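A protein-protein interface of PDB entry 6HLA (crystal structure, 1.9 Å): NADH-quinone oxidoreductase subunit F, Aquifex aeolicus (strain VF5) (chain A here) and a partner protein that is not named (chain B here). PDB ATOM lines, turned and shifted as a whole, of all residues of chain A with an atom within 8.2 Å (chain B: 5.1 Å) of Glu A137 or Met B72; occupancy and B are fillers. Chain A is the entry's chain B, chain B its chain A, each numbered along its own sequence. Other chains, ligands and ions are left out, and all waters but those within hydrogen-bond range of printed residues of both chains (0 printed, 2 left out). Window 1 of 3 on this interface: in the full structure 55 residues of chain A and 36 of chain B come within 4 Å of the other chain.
Of the printed residues of chain B, Glu A137 touches Met B72, Leu B128 and Met B138. Met B72 touches just these residues of chain A: Gly A136, Glu A137, Ala A177 and Gly A178. Of the printed residues of chain A, Leu B128 touches Arg A104 (3.6 Å), Arg A135 (3.5 Å), Glu A137 (3.8 Å) and Tyr A138 (3.6 Å). Of the printed residues of chain A, Met B138 touches Glu A137 and Pro A139. Glu A95 touches none of the printed residues of chain B. Ala A93 touches none of the printed residues of chain B. The nearest residue of chain B that does not touch Glu A137 is Glu B143 (4.5 Å).
OD2 of Asp B71 is in hydrogen-bond range of NE2 of His A344, at 3.2 Å. The backbone carbonyl oxygen (O) of Ala A177 lies within hydrogen-bond range of the backbone NH (N) of Met B72. OE1 of Glu B143 is in salt-bridge range of NH1 of Arg A104, 2.8 Å away. The side-chain sulfur (SD) of Met B72 sits close to the side-chain carboxylate (OE2) of Glu A137, at 3.8 Å. The backbone NH (N) of Glu B143 is in hydrogen-bond range of the backbone carbonyl oxygen (O) of Ala A6 (2.9 Å). NE2 of His B35 lies within hydrogen-bond range of O of Gly A176 (3.0 Å). The backbone carbonyl oxygen (O) of Ala A177 sits at hydrogen-bond distance from the backbone NH (N) of Asp B71 (3.4 Å).
Among the printed residues, pairs that only touch across the chains: Ala A177 with Tyr B70 (3.3 Å), Arg A135 with Leu B128 (3.5 Å), Ala A177 with Phe B73 (3.6 Å), Arg A104 with Leu B128 (3.6 Å), Tyr A138 with Leu B128 (3.6 Å), Glu A137 with Met B138 (3.6 Å), Gly A136 with Met B72 (3.6 Å), Gly A178 with Met B72 (3.7 Å), Arg A175 with His B35 (3.7 Å), Ala A177 with His B35 (3.8 Å), Glu A137 with Leu B128 (3.8 Å), Pro A139 with Met B138 (3.9 Å) and Gly A178 with Asp B71 (3.9 Å).
The backbone NH (N) of Met B138 is in hydrogen-bond range of the backbone carbonyl oxygen (O) of Arg B84 (2.8 Å). NE2 of Gln B38 lies within hydrogen-bond range of O of Met B72, 2.8 Å away. OH of Tyr A138 sits at hydrogen-bond distance from OE1 of Glu A95 (2.7 Å). The side-chain carboxylate of Glu A108 lies within salt-bridge range of the guanidinium group of Arg A104 (3.0 Å). NH1 of Arg A135 lies within hydrogen-bond range of O of Glu A95. OE1 of Glu A95 is in hydrogen-bond range of N of Arg A104, at 3.1 Å.
Of the 11 printed residues of chain B, 8 touch a printed residue of chain A. Printed residues of chain B that touch a printed residue of chain A: His B35, Tyr B70, Asp B71, Met B72, Phe B73, Leu B128, Met B138 and Glu B143. Hydrophobic or aromatic side chains of chain B that line the printed part of chain A: His B35, Tyr B70, Met B72, Phe B73, Leu B128 and Met B138. Along chain B the printed residues that touch a printed residue of chain A span positions 35 to 143. Along chain A the printed residues that touch a printed residue of chain B span positions 6 to 344. Among the printed residues, 20 pairs touch across the chains.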
ATOM      1  N   ALA A   6     -25.458   5.156  30.336  1.00  0.00           N
ATOM      2  CA  ALA A   6     -25.145   5.836  31.596  1.00  0.00           C
ATOM      3  C   ALA A   6     -25.469   7.318  31.541  1.00  0.00           C
ATOM      4  O   ALA A   6     -25.184   7.985  30.533  1.00  0.00           O
ATOM      5  CB  ALA A   6     -23.682   5.636  31.948  1.00  0.00           C
ATOM      6  N   ILE A   7     -26.109   7.837  32.608  1.00  0.00           N
ATOM      7  CA  ILE A   7     -26.445   9.257  32.700  1.00  0.00           C
ATOM      8  C   ILE A   7     -26.004   9.801  34.054  1.00  0.00           C
ATOM      9  O   ILE A   7     -26.271   9.173  35.079  1.00  0.00           O
ATOM     10  CB  ILE A   7     -27.903   9.662  32.327  1.00  0.00           C
ATOM     11  CG1 ILE A   7     -28.954   8.650  32.819  1.00  0.00           C
ATOM     12  CG2 ILE A   7     -28.002   9.907  30.833  1.00  0.00           C
ATOM     13  CD1 ILE A   7     -30.367   8.822  32.278  1.00  0.00           C
ATOM     14  N   ALA A  93     -37.684  19.153  22.935  1.00  0.00           N
ATOM     15  CA  ALA A  93     -36.739  18.583  23.891  1.00  0.00           C
ATOM     16  C   ALA A  93     -35.316  18.742  23.387  1.00  0.00           C
ATOM     17  O   ALA A  93     -34.446  17.944  23.721  1.00  0.00           O
ATOM     18  CB  ALA A  93     -37.074  17.112  24.176  1.00  0.00           C
ATOM     19  N   ASP A  94     -35.063  19.823  22.616  1.00  0.00           N
ATOM     20  CA  ASP A  94     -33.749  20.051  22.055  1.00  0.00           C
ATOM     21  C   ASP A  94     -32.718  20.565  23.056  1.00  0.00           C
ATOM     22  O   ASP A  94     -31.532  20.429  22.773  1.00  0.00           O
ATOM     23  CB  ASP A  94     -33.778  20.947  20.795  1.00  0.00           C
ATOM     24  CG  ASP A  94     -32.512  20.785  19.986  1.00  0.00           C
ATOM     25  OD1 ASP A  94     -32.280  19.660  19.472  1.00  0.00           O
ATOM     26  OD2 ASP A  94     -31.646  21.696  20.049  1.00  0.00           O
ATOM     27  N   GLU A  95     -33.151  21.112  24.206  1.00  0.00           N
ATOM     28  CA  GLU A  95     -32.347  21.693  25.303  1.00  0.00           C
ATOM     29  C   GLU A  95     -30.848  21.722  25.016  1.00  0.00           C
ATOM     30  O   GLU A  95     -30.152  20.723  25.265  1.00  0.00           O
ATOM     31  CB  GLU A  95     -32.638  20.946  26.614  1.00  0.00           C
ATOM     32  CG  GLU A  95     -31.924  21.542  27.797  1.00  0.00           C
ATOM     33  CD  GLU A  95     -32.436  21.002  29.105  1.00  0.00           C
ATOM     34  OE1 GLU A  95     -32.282  19.788  29.329  1.00  0.00           O
ATOM     35  OE2 GLU A  95     -33.060  21.773  29.868  1.00  0.00           O
ATOM     36  N   SER A  96     -30.363  22.818  24.397  1.00  0.00           N
ATOM     37  CA  SER A  96     -28.955  22.898  24.035  1.00  0.00           C
ATOM     38  C   SER A  96     -28.265  24.191  24.485  1.00  0.00           C
ATOM     39  O   SER A  96     -27.086  24.398  24.188  1.00  0.00           O
ATOM     40  CB  SER A  96     -28.789  22.665  22.540  1.00  0.00           C
ATOM     41  OG  SER A  96     -29.026  21.303  22.228  1.00  0.00           O
ATOM     42  N   ARG A 104     -34.096  17.673  30.699  1.00  0.00           N
ATOM     43  CA  ARG A 104     -33.625  16.287  30.683  1.00  0.00           C
ATOM     44  C   ARG A 104     -34.012  15.498  31.952  1.00  0.00           C
ATOM     45  O   ARG A 104     -34.290  14.309  31.831  1.00  0.00           O
ATOM     46  CB  ARG A 104     -32.103  16.244  30.446  1.00  0.00           C
ATOM     47  CG  ARG A 104     -31.251  16.508  31.689  1.00  0.00           C
ATOM     48  CD  ARG A 104     -29.782  16.283  31.425  1.00  0.00           C
ATOM     49  NE  ARG A 104     -29.478  14.903  31.022  1.00  0.00           N
ATOM     50  CZ  ARG A 104     -28.347  14.526  30.432  1.00  0.00           C
ATOM     51  NH1 ARG A 104     -27.386  15.408  30.195  1.00  0.00           N
ATOM     52  NH2 ARG A 104     -28.186  13.278  30.039  1.00  0.00           N
ATOM     53  N   GLU A 108     -35.914  12.009  31.586  1.00  0.00           N
ATOM     54  CA  GLU A 108     -35.212  10.816  32.046  1.00  0.00           C
ATOM     55  C   GLU A 108     -35.775  10.205  33.330  1.00  0.00           C
ATOM     56  O   GLU A 108     -35.610   9.014  33.529  1.00  0.00           O
ATOM     57  CB  GLU A 108     -33.717  11.123  32.205  1.00  0.00           C
ATOM     58  CG  GLU A 108     -33.039  11.455  30.876  1.00  0.00           C
ATOM     59  CD  GLU A 108     -31.695  12.160  30.947  1.00  0.00           C
ATOM     60  OE1 GLU A 108     -31.309  12.630  32.041  1.00  0.00           O
ATOM     61  OE2 GLU A 108     -31.030  12.261  29.894  1.00  0.00           O
ATOM     62  N   ILE A 134     -36.030  15.410  20.360  1.00  0.00           N
ATOM     63  CA  ILE A 134     -35.034  15.401  21.445  1.00  0.00           C
ATOM     64  C   ILE A 134     -33.626  15.497  20.889  1.00  0.00           C
ATOM     65  O   ILE A 134     -33.295  14.760  19.958  1.00  0.00           O
ATOM     66  CB  ILE A 134     -35.243  14.205  22.427  1.00  0.00           C
ATOM     67  CG1 ILE A 134     -34.325  14.321  23.682  1.00  0.00           C
ATOM     68  CG2 ILE A 134     -35.100  12.811  21.708  1.00  0.00           C
ATOM     69  CD1 ILE A 134     -34.685  13.300  24.896  1.00  0.00           C
ATOM     70  N   ARG A 135     -32.760  16.344  21.500  1.00  0.00           N
ATOM     71  CA  ARG A 135     -31.392  16.489  21.003  1.00  0.00           C
ATOM     72  C   ARG A 135     -30.699  15.122  20.920  1.00  0.00           C
ATOM     73  O   ARG A 135     -30.997  14.222  21.720  1.00  0.00           O
ATOM     74  CB  ARG A 135     -30.589  17.484  21.853  1.00  0.00           C
ATOM     75  CG  ARG A 135     -30.299  16.991  23.276  1.00  0.00           C
ATOM     76  CD  ARG A 135     -29.485  17.982  24.065  1.00  0.00           C
ATOM     77  NE  ARG A 135     -28.143  18.197  23.518  1.00  0.00           N
ATOM     78  CZ  ARG A 135     -27.244  19.024  24.043  1.00  0.00           C
ATOM     79  NH1 ARG A 135     -27.540  19.739  25.117  1.00  0.00           N
ATOM     80  NH2 ARG A 135     -26.046  19.144  23.493  1.00  0.00           N
ATOM     81  N   GLY A 136     -29.854  14.944  19.920  1.00  0.00           N
ATOM     82  CA  GLY A 136     -29.165  13.673  19.706  1.00  0.00           C
ATOM     83  C   GLY A 136     -28.204  13.296  20.813  1.00  0.00           C
ATOM     84  O   GLY A 136     -27.832  12.121  20.935  1.00  0.00           O
ATOM     85  N   GLU A 137     -27.798  14.284  21.639  1.00  0.00           N
ATOM     86  CA  GLU A 137     -26.840  14.078  22.746  1.00  0.00           C
ATOM     87  C   GLU A 137     -27.539  13.616  24.015  1.00  0.00           C
ATOM     88  O   GLU A 137     -26.892  13.391  25.034  1.00  0.00           O
ATOM     89  CB  GLU A 137     -25.929  15.291  22.983  1.00  0.00           C
ATOM     90  CG  GLU A 137     -25.198  15.763  21.736  1.00  0.00           C
ATOM     91  CD  GLU A 137     -25.937  16.718  20.824  1.00  0.00           C
ATOM     92  OE1 GLU A 137     -27.126  17.008  21.078  1.00  0.00           O
ATOM     93  OE2 GLU A 137     -25.317  17.183  19.844  1.00  0.00           O
ATOM     94  N   TYR A 138     -28.843  13.344  23.905  1.00  0.00           N
ATOM     95  CA  TYR A 138     -29.678  12.787  24.979  1.00  0.00           C
ATOM     96  C   TYR A 138     -30.138  11.404  24.519  1.00  0.00           C
ATOM     97  O   TYR A 138     -31.343  11.203  24.348  1.00  0.00           O
ATOM     98  CB  TYR A 138     -30.908  13.688  25.234  1.00  0.00           C
ATOM     99  CG  TYR A 138     -30.704  14.934  26.073  1.00  0.00           C
ATOM    100  CD1 TYR A 138     -29.472  15.214  26.662  1.00  0.00           C
ATOM    101  CD2 TYR A 138     -31.744  15.835  26.284  1.00  0.00           C
ATOM    102  CE1 TYR A 138     -29.280  16.367  27.426  1.00  0.00           C
ATOM    103  CE2 TYR A 138     -31.553  17.003  27.024  1.00  0.00           C
ATOM    104  CZ  TYR A 138     -30.321  17.254  27.605  1.00  0.00           C
ATOM    105  OH  TYR A 138     -30.142  18.374  28.367  1.00  0.00           O
ATOM    106  N   PRO A 139     -29.228  10.426  24.253  1.00  0.00           N
ATOM    107  CA  PRO A 139     -29.701   9.125  23.782  1.00  0.00           C
ATOM    108  C   PRO A 139     -30.488   8.347  24.824  1.00  0.00           C
ATOM    109  O   PRO A 139     -31.458   7.691  24.456  1.00  0.00           O
ATOM    110  CB  PRO A 139     -28.410   8.396  23.387  1.00  0.00           C
ATOM    111  CG  PRO A 139     -27.335   9.033  24.210  1.00  0.00           C
ATOM    112  CD  PRO A 139     -27.758  10.452  24.375  1.00  0.00           C
ATOM    113  N   ALA A 140     -30.099   8.443  26.131  1.00  0.00           N
ATOM    114  CA  ALA A 140     -30.814   7.729  27.199  1.00  0.00           C
ATOM    115  C   ALA A 140     -32.234   8.282  27.283  1.00  0.00           C
ATOM    116  O   ALA A 140     -33.174   7.501  27.292  1.00  0.00           O
ATOM    117  CB  ALA A 140     -30.087   7.877  28.545  1.00  0.00           C
ATOM    118  N   GLY A 141     -32.371   9.604  27.234  1.00  0.00           N
ATOM    119  CA  GLY A 141     -33.678  10.260  27.225  1.00  0.00           C
ATOM    120  C   GLY A 141     -34.545   9.751  26.083  1.00  0.00           C
ATOM    121  O   GLY A 141     -35.737   9.484  26.275  1.00  0.00           O
ATOM    122  N   TYR A 142     -33.920   9.499  24.903  1.00  0.00           N
ATOM    123  CA  TYR A 142     -34.629   8.975  23.734  1.00  0.00           C
ATOM    124  C   TYR A 142     -35.176   7.558  23.976  1.00  0.00           C
ATOM    125  O   TYR A 142     -36.347   7.322  23.690  1.00  0.00           O
ATOM    126  CB  TYR A 142     -33.763   9.041  22.459  1.00  0.00           C
ATOM    127  CG  TYR A 142     -34.323   8.237  21.302  1.00  0.00           C
ATOM    128  CD1 TYR A 142     -35.383   8.719  20.540  1.00  0.00           C
ATOM    129  CD2 TYR A 142     -33.822   6.971  20.999  1.00  0.00           C
ATOM    130  CE1 TYR A 142     -35.901   7.980  19.472  1.00  0.00           C
ATOM    131  CE2 TYR A 142     -34.349   6.217  19.955  1.00  0.00           C
ATOM    132  CZ  TYR A 142     -35.388   6.727  19.194  1.00  0.00           C
ATOM    133  OH  TYR A 142     -35.891   5.968  18.167  1.00  0.00           O
ATOM    134  N   ARG A 175     -34.988  12.445  16.832  1.00  0.00           N
ATOM    135  CA  ARG A 175     -33.716  12.831  17.433  1.00  0.00           C
ATOM    136  C   ARG A 175     -33.039  13.912  16.613  1.00  0.00           C
ATOM    137  O   ARG A 175     -33.038  13.855  15.390  1.00  0.00           O
ATOM    138  CB  ARG A 175     -32.752  11.623  17.545  1.00  0.00           C
ATOM    139  CG  ARG A 175     -33.180  10.537  18.514  1.00  0.00           C
ATOM    140  CD  ARG A 175     -32.145   9.429  18.577  1.00  0.00           C
ATOM    141  NE  ARG A 175     -30.978   9.809  19.380  1.00  0.00           N
ATOM    142  CZ  ARG A 175     -29.815   9.174  19.362  1.00  0.00           C
ATOM    143  NH1 ARG A 175     -29.636   8.126  18.572  1.00  0.00           N
ATOM    144  NH2 ARG A 175     -28.811   9.589  20.127  1.00  0.00           N
ATOM    145  N   GLY A 176     -32.421  14.858  17.301  1.00  0.00           N
ATOM    146  CA  GLY A 176     -31.584  15.877  16.686  1.00  0.00           C
ATOM    147  C   GLY A 176     -30.260  15.234  16.342  1.00  0.00           C
ATOM    148  O   GLY A 176     -30.082  14.042  16.607  1.00  0.00           O
ATOM    149  N   ALA A 177     -29.306  15.986  15.769  1.00  0.00           N
ATOM    150  CA  ALA A 177     -28.013  15.378  15.447  1.00  0.00           C
ATOM    151  C   ALA A 177     -26.822  16.351  15.519  1.00  0.00           C
ATOM    152  O   ALA A 177     -25.928  16.286  14.693  1.00  0.00           O
ATOM    153  CB  ALA A 177     -28.072  14.670  14.105  1.00  0.00           C
ATOM    154  N   GLY A 178     -26.795  17.177  16.556  1.00  0.00           N
ATOM    155  CA  GLY A 178     -25.692  18.092  16.834  1.00  0.00           C
ATOM    156  C   GLY A 178     -25.920  19.590  16.734  1.00  0.00           C
ATOM    157  O   GLY A 178     -25.056  20.365  17.165  1.00  0.00           O
ATOM    158  N   ALA A 179     -27.048  20.020  16.156  1.00  0.00           N
ATOM    159  CA  ALA A 179     -27.297  21.441  15.903  1.00  0.00           C
ATOM    160  C   ALA A 179     -28.128  22.153  16.957  1.00  0.00           C
ATOM    161  O   ALA A 179     -29.271  21.774  17.186  1.00  0.00           O
ATOM    162  CB  ALA A 179     -27.929  21.616  14.519  1.00  0.00           C
ATOM    163  N   TYR A 180     -27.541  23.173  17.618  1.00  0.00           N
ATOM    164  CA  TYR A 180     -28.211  23.988  18.642  1.00  0.00           C
ATOM    165  C   TYR A 180     -29.415  24.725  18.054  1.00  0.00           C
ATOM    166  O   TYR A 180     -30.445  24.856  18.707  1.00  0.00           O
ATOM    167  CB  TYR A 180     -27.204  24.961  19.257  1.00  0.00           C
ATOM    168  CG  TYR A 180     -27.765  26.179  19.952  1.00  0.00           C
ATOM    169  CD1 TYR A 180     -28.263  26.101  21.255  1.00  0.00           C
ATOM    170  CD2 TYR A 180     -27.708  27.429  19.351  1.00  0.00           C
ATOM    171  CE1 TYR A 180     -28.707  27.235  21.925  1.00  0.00           C
ATOM    172  CE2 TYR A 180     -28.152  28.570  20.013  1.00  0.00           C
ATOM    173  CZ  TYR A 180     -28.648  28.471  21.299  1.00  0.00           C
ATOM    174  OH  TYR A 180     -29.045  29.622  21.938  1.00  0.00           O
ATOM    175  N   HIS A 344     -19.832  28.350  16.476  1.00  0.00           N
ATOM    176  CA  HIS A 344     -20.119  26.955  16.153  1.00  0.00           C
ATOM    177  C   HIS A 344     -21.593  26.679  15.775  1.00  0.00           C
ATOM    178  O   HIS A 344     -21.861  25.729  15.040  1.00  0.00           O
ATOM    179  CB  HIS A 344     -19.671  26.039  17.327  1.00  0.00           C
ATOM    180  CG  HIS A 344     -19.659  24.576  16.973  1.00  0.00           C
ATOM    181  ND1 HIS A 344     -18.620  24.002  16.243  1.00  0.00           N
ATOM    182  CD2 HIS A 344     -20.621  23.639  17.164  1.00  0.00           C
ATOM    183  CE1 HIS A 344     -18.986  22.748  16.019  1.00  0.00           C
ATOM    184  NE2 HIS A 344     -20.164  22.467  16.586  1.00  0.00           N
ATOM    185  N   GLU A 345     -22.536  27.527  16.229  1.00  0.00           N
ATOM    186  CA  GLU A 345     -23.968  27.247  16.071  1.00  0.00           C
ATOM    187  C   GLU A 345     -24.764  28.067  15.028  1.00  0.00           C
ATOM    188  O   GLU A 345     -25.895  27.676  14.704  1.00  0.00           O
ATOM    189  CB  GLU A 345     -24.664  27.332  17.437  1.00  0.00           C
ATOM    190  CG  GLU A 345     -24.076  26.362  18.448  1.00  0.00           C
ATOM    191  CD  GLU A 345     -23.974  24.898  18.047  1.00  0.00           C
ATOM    192  OE1 GLU A 345     -24.773  24.434  17.203  1.00  0.00           O
ATOM    193  OE2 GLU A 345     -23.130  24.194  18.640  1.00  0.00           O
ATOM    194  N   HIS B  35     -27.918   8.004  12.328  1.00  0.00           N
ATOM    195  CA  HIS B  35     -27.437   7.636  13.674  1.00  0.00           C
ATOM    196  C   HIS B  35     -27.149   6.122  13.702  1.00  0.00           C
ATOM    197  O   HIS B  35     -26.109   5.705  14.216  1.00  0.00           O
ATOM    198  CB  HIS B  35     -28.482   7.979  14.752  1.00  0.00           C
ATOM    199  CG  HIS B  35     -28.409   9.388  15.277  1.00  0.00           C
ATOM    200  ND1 HIS B  35     -27.270   9.870  15.887  1.00  0.00           N
ATOM    201  CD2 HIS B  35     -29.365  10.348  15.319  1.00  0.00           C
ATOM    202  CE1 HIS B  35     -27.559  11.109  16.271  1.00  0.00           C
ATOM    203  NE2 HIS B  35     -28.799  11.446  15.939  1.00  0.00           N
ATOM    204  N   GLN B  38     -24.042   5.220  11.605  1.00  0.00           N
ATOM    205  CA  GLN B  38     -22.852   5.553  12.393  1.00  0.00           C
ATOM    206  C   GLN B  38     -22.649   4.594  13.581  1.00  0.00           C
ATOM    207  O   GLN B  38     -21.503   4.274  13.916  1.00  0.00           O
ATOM    208  CB  GLN B  38     -22.864   7.023  12.836  1.00  0.00           C
ATOM    209  CG  GLN B  38     -21.552   7.452  13.481  1.00  0.00           C
ATOM    210  CD  GLN B  38     -21.245   8.904  13.320  1.00  0.00           C
ATOM    211  OE1 GLN B  38     -21.041   9.409  12.210  1.00  0.00           O
ATOM    212  NE2 GLN B  38     -21.118   9.580  14.447  1.00  0.00           N
ATOM    213  N   TYR B  70     -25.357  18.240  10.083  1.00  0.00           N
ATOM    214  CA  TYR B  70     -25.445  17.702  11.446  1.00  0.00           C
ATOM    215  C   TYR B  70     -24.118  17.163  11.965  1.00  0.00           C
ATOM    216  O   TYR B  70     -23.630  16.131  11.499  1.00  0.00           O
ATOM    217  CB  TYR B  70     -26.572  16.685  11.510  1.00  0.00           C
ATOM    218  CG  TYR B  70     -27.939  17.306  11.297  1.00  0.00           C
ATOM    219  CD1 TYR B  70     -28.588  17.202  10.073  1.00  0.00           C
ATOM    220  CD2 TYR B  70     -28.566  18.031  12.307  1.00  0.00           C
ATOM    221  CE1 TYR B  70     -29.851  17.758   9.870  1.00  0.00           C
ATOM    222  CE2 TYR B  70     -29.834  18.584  12.120  1.00  0.00           C
ATOM    223  CZ  TYR B  70     -30.474  18.446  10.896  1.00  0.00           C
ATOM    224  OH  TYR B  70     -31.708  19.013  10.671  1.00  0.00           O
ATOM    225  N   ASP B  71     -23.549  17.895  12.958  1.00  0.00           N
ATOM    226  CA  ASP B  71     -22.216  17.703  13.551  1.00  0.00           C
ATOM    227  C   ASP B  71     -21.957  16.358  14.244  1.00  0.00           C
ATOM    228  O   ASP B  71     -20.792  16.004  14.435  1.00  0.00           O
ATOM    229  CB  ASP B  71     -21.862  18.850  14.515  1.00  0.00           C
ATOM    230  CG  ASP B  71     -21.802  20.240  13.886  1.00  0.00           C
ATOM    231  OD1 ASP B  71     -21.234  20.378  12.775  1.00  0.00           O
ATOM    232  OD2 ASP B  71     -22.249  21.195  14.535  1.00  0.00           O
ATOM    233  N   MET B  72     -23.005  15.609  14.613  1.00  0.00           N
ATOM    234  CA  MET B  72     -22.794  14.315  15.266  1.00  0.00           C
ATOM    235  C   MET B  72     -22.260  13.274  14.286  1.00  0.00           C
ATOM    236  O   MET B  72     -21.609  12.310  14.713  1.00  0.00           O
ATOM    237  CB  MET B  72     -24.077  13.818  15.942  1.00  0.00           C
ATOM    238  CG  MET B  72     -24.347  14.510  17.264  1.00  0.00           C
ATOM    239  SD  MET B  72     -25.698  13.772  18.229  1.00  0.00           S
ATOM    240  CE  MET B  72     -24.907  12.250  18.819  1.00  0.00           C
ATOM    241  N   PHE B  73     -22.521  13.498  12.971  1.00  0.00           N
ATOM    242  CA  PHE B  73     -22.144  12.631  11.846  1.00  0.00           C
ATOM    243  C   PHE B  73     -20.745  12.902  11.332  1.00  0.00           C
ATOM    244  O   PHE B  73     -20.399  14.050  11.050  1.00  0.00           O
ATOM    245  CB  PHE B  73     -23.185  12.715  10.711  1.00  0.00           C
ATOM    246  CG  PHE B  73     -24.607  12.444  11.150  1.00  0.00           C
ATOM    247  CD1 PHE B  73     -24.897  11.402  12.034  1.00  0.00           C
ATOM    248  CD2 PHE B  73     -25.657  13.213  10.670  1.00  0.00           C
ATOM    249  CE1 PHE B  73     -26.202  11.170  12.467  1.00  0.00           C
ATOM    250  CE2 PHE B  73     -26.972  12.962  11.084  1.00  0.00           C
ATOM    251  CZ  PHE B  73     -27.232  11.945  11.989  1.00  0.00           C
ATOM    252  N   ASP B  74     -19.938  11.824  11.222  1.00  0.00           N
ATOM    253  CA  ASP B  74     -18.543  11.877  10.801  1.00  0.00           C
ATOM    254  C   ASP B  74     -18.335  10.926   9.633  1.00  0.00           C
ATOM    255  O   ASP B  74     -18.455   9.712   9.784  1.00  0.00           O
ATOM    256  CB  ASP B  74     -17.627  11.548  12.010  1.00  0.00           C
ATOM    257  CG  ASP B  74     -16.129  11.369  11.781  1.00  0.00           C
ATOM    258  OD1 ASP B  74     -15.634  11.727  10.678  1.00  0.00           O
ATOM    259  OD2 ASP B  74     -15.448  10.898  12.711  1.00  0.00           O
ATOM    260  N   ARG B  84     -16.830  12.218  23.449  1.00  0.00           N
ATOM    261  CA  ARG B  84     -17.314  13.587  23.237  1.00  0.00           C
ATOM    262  C   ARG B  84     -16.961  14.412  24.450  1.00  0.00           C
ATOM    263  O   ARG B  84     -17.375  14.074  25.557  1.00  0.00           O
ATOM    264  CB  ARG B  84     -18.813  13.613  22.933  1.00  0.00           C
ATOM    265  CG  ARG B  84     -19.105  13.209  21.497  1.00  0.00           C
ATOM    266  CD  ARG B  84     -20.574  13.158  21.187  1.00  0.00           C
ATOM    267  NE  ARG B  84     -20.989  11.845  20.680  1.00  0.00           N
ATOM    268  CZ  ARG B  84     -21.099  11.531  19.391  1.00  0.00           C
ATOM    269  NH1 ARG B  84     -20.809  12.426  18.454  1.00  0.00           N
ATOM    270  NH2 ARG B  84     -21.509  10.324  19.030  1.00  0.00           N
ATOM    271  N   LEU B 128     -23.353  19.838  26.588  1.00  0.00           N
ATOM    272  CA  LEU B 128     -24.069  18.566  26.562  1.00  0.00           C
ATOM    273  C   LEU B 128     -25.268  18.491  27.509  1.00  0.00           C
ATOM    274  O   LEU B 128     -25.848  17.424  27.680  1.00  0.00           O
ATOM    275  CB  LEU B 128     -23.074  17.402  26.856  1.00  0.00           C
ATOM    276  CG  LEU B 128     -22.014  17.105  25.801  1.00  0.00           C
ATOM    277  CD1 LEU B 128     -20.872  16.272  26.400  1.00  0.00           C
ATOM    278  CD2 LEU B 128     -22.616  16.393  24.594  1.00  0.00           C
ATOM    279  N   MET B 138     -18.813  12.185  27.088  1.00  0.00           N
ATOM    280  CA  MET B 138     -19.600  11.024  26.674  1.00  0.00           C
ATOM    281  C   MET B 138     -18.634   9.995  26.081  1.00  0.00           C
ATOM    282  O   MET B 138     -17.590  10.380  25.565  1.00  0.00           O
ATOM    283  CB  MET B 138     -20.644  11.412  25.610  1.00  0.00           C
ATOM    284  CG  MET B 138     -21.701  12.378  26.111  1.00  0.00           C
ATOM    285  SD  MET B 138     -23.074  12.557  24.952  1.00  0.00           S
ATOM    286  CE  MET B 138     -24.099  11.150  25.405  1.00  0.00           C
ATOM    287  N   GLU B 143     -22.725   8.829  29.349  1.00  0.00           N
ATOM    288  CA  GLU B 143     -22.294  10.166  29.778  1.00  0.00           C
ATOM    289  C   GLU B 143     -21.838  10.161  31.245  1.00  0.00           C
ATOM    290  O   GLU B 143     -22.487   9.533  32.105  1.00  0.00           O
ATOM    291  CB  GLU B 143     -23.424  11.160  29.595  1.00  0.00           C
ATOM    292  CG  GLU B 143     -23.018  12.582  29.916  1.00  0.00           C
ATOM    293  CD  GLU B 143     -24.026  13.562  29.402  1.00  0.00           C
ATOM    294  OE1 GLU B 143     -25.043  13.794  30.092  1.00  0.00           O
ATOM    295  OE2 GLU B 143     -23.847  14.009  28.250  1.00  0.00           O
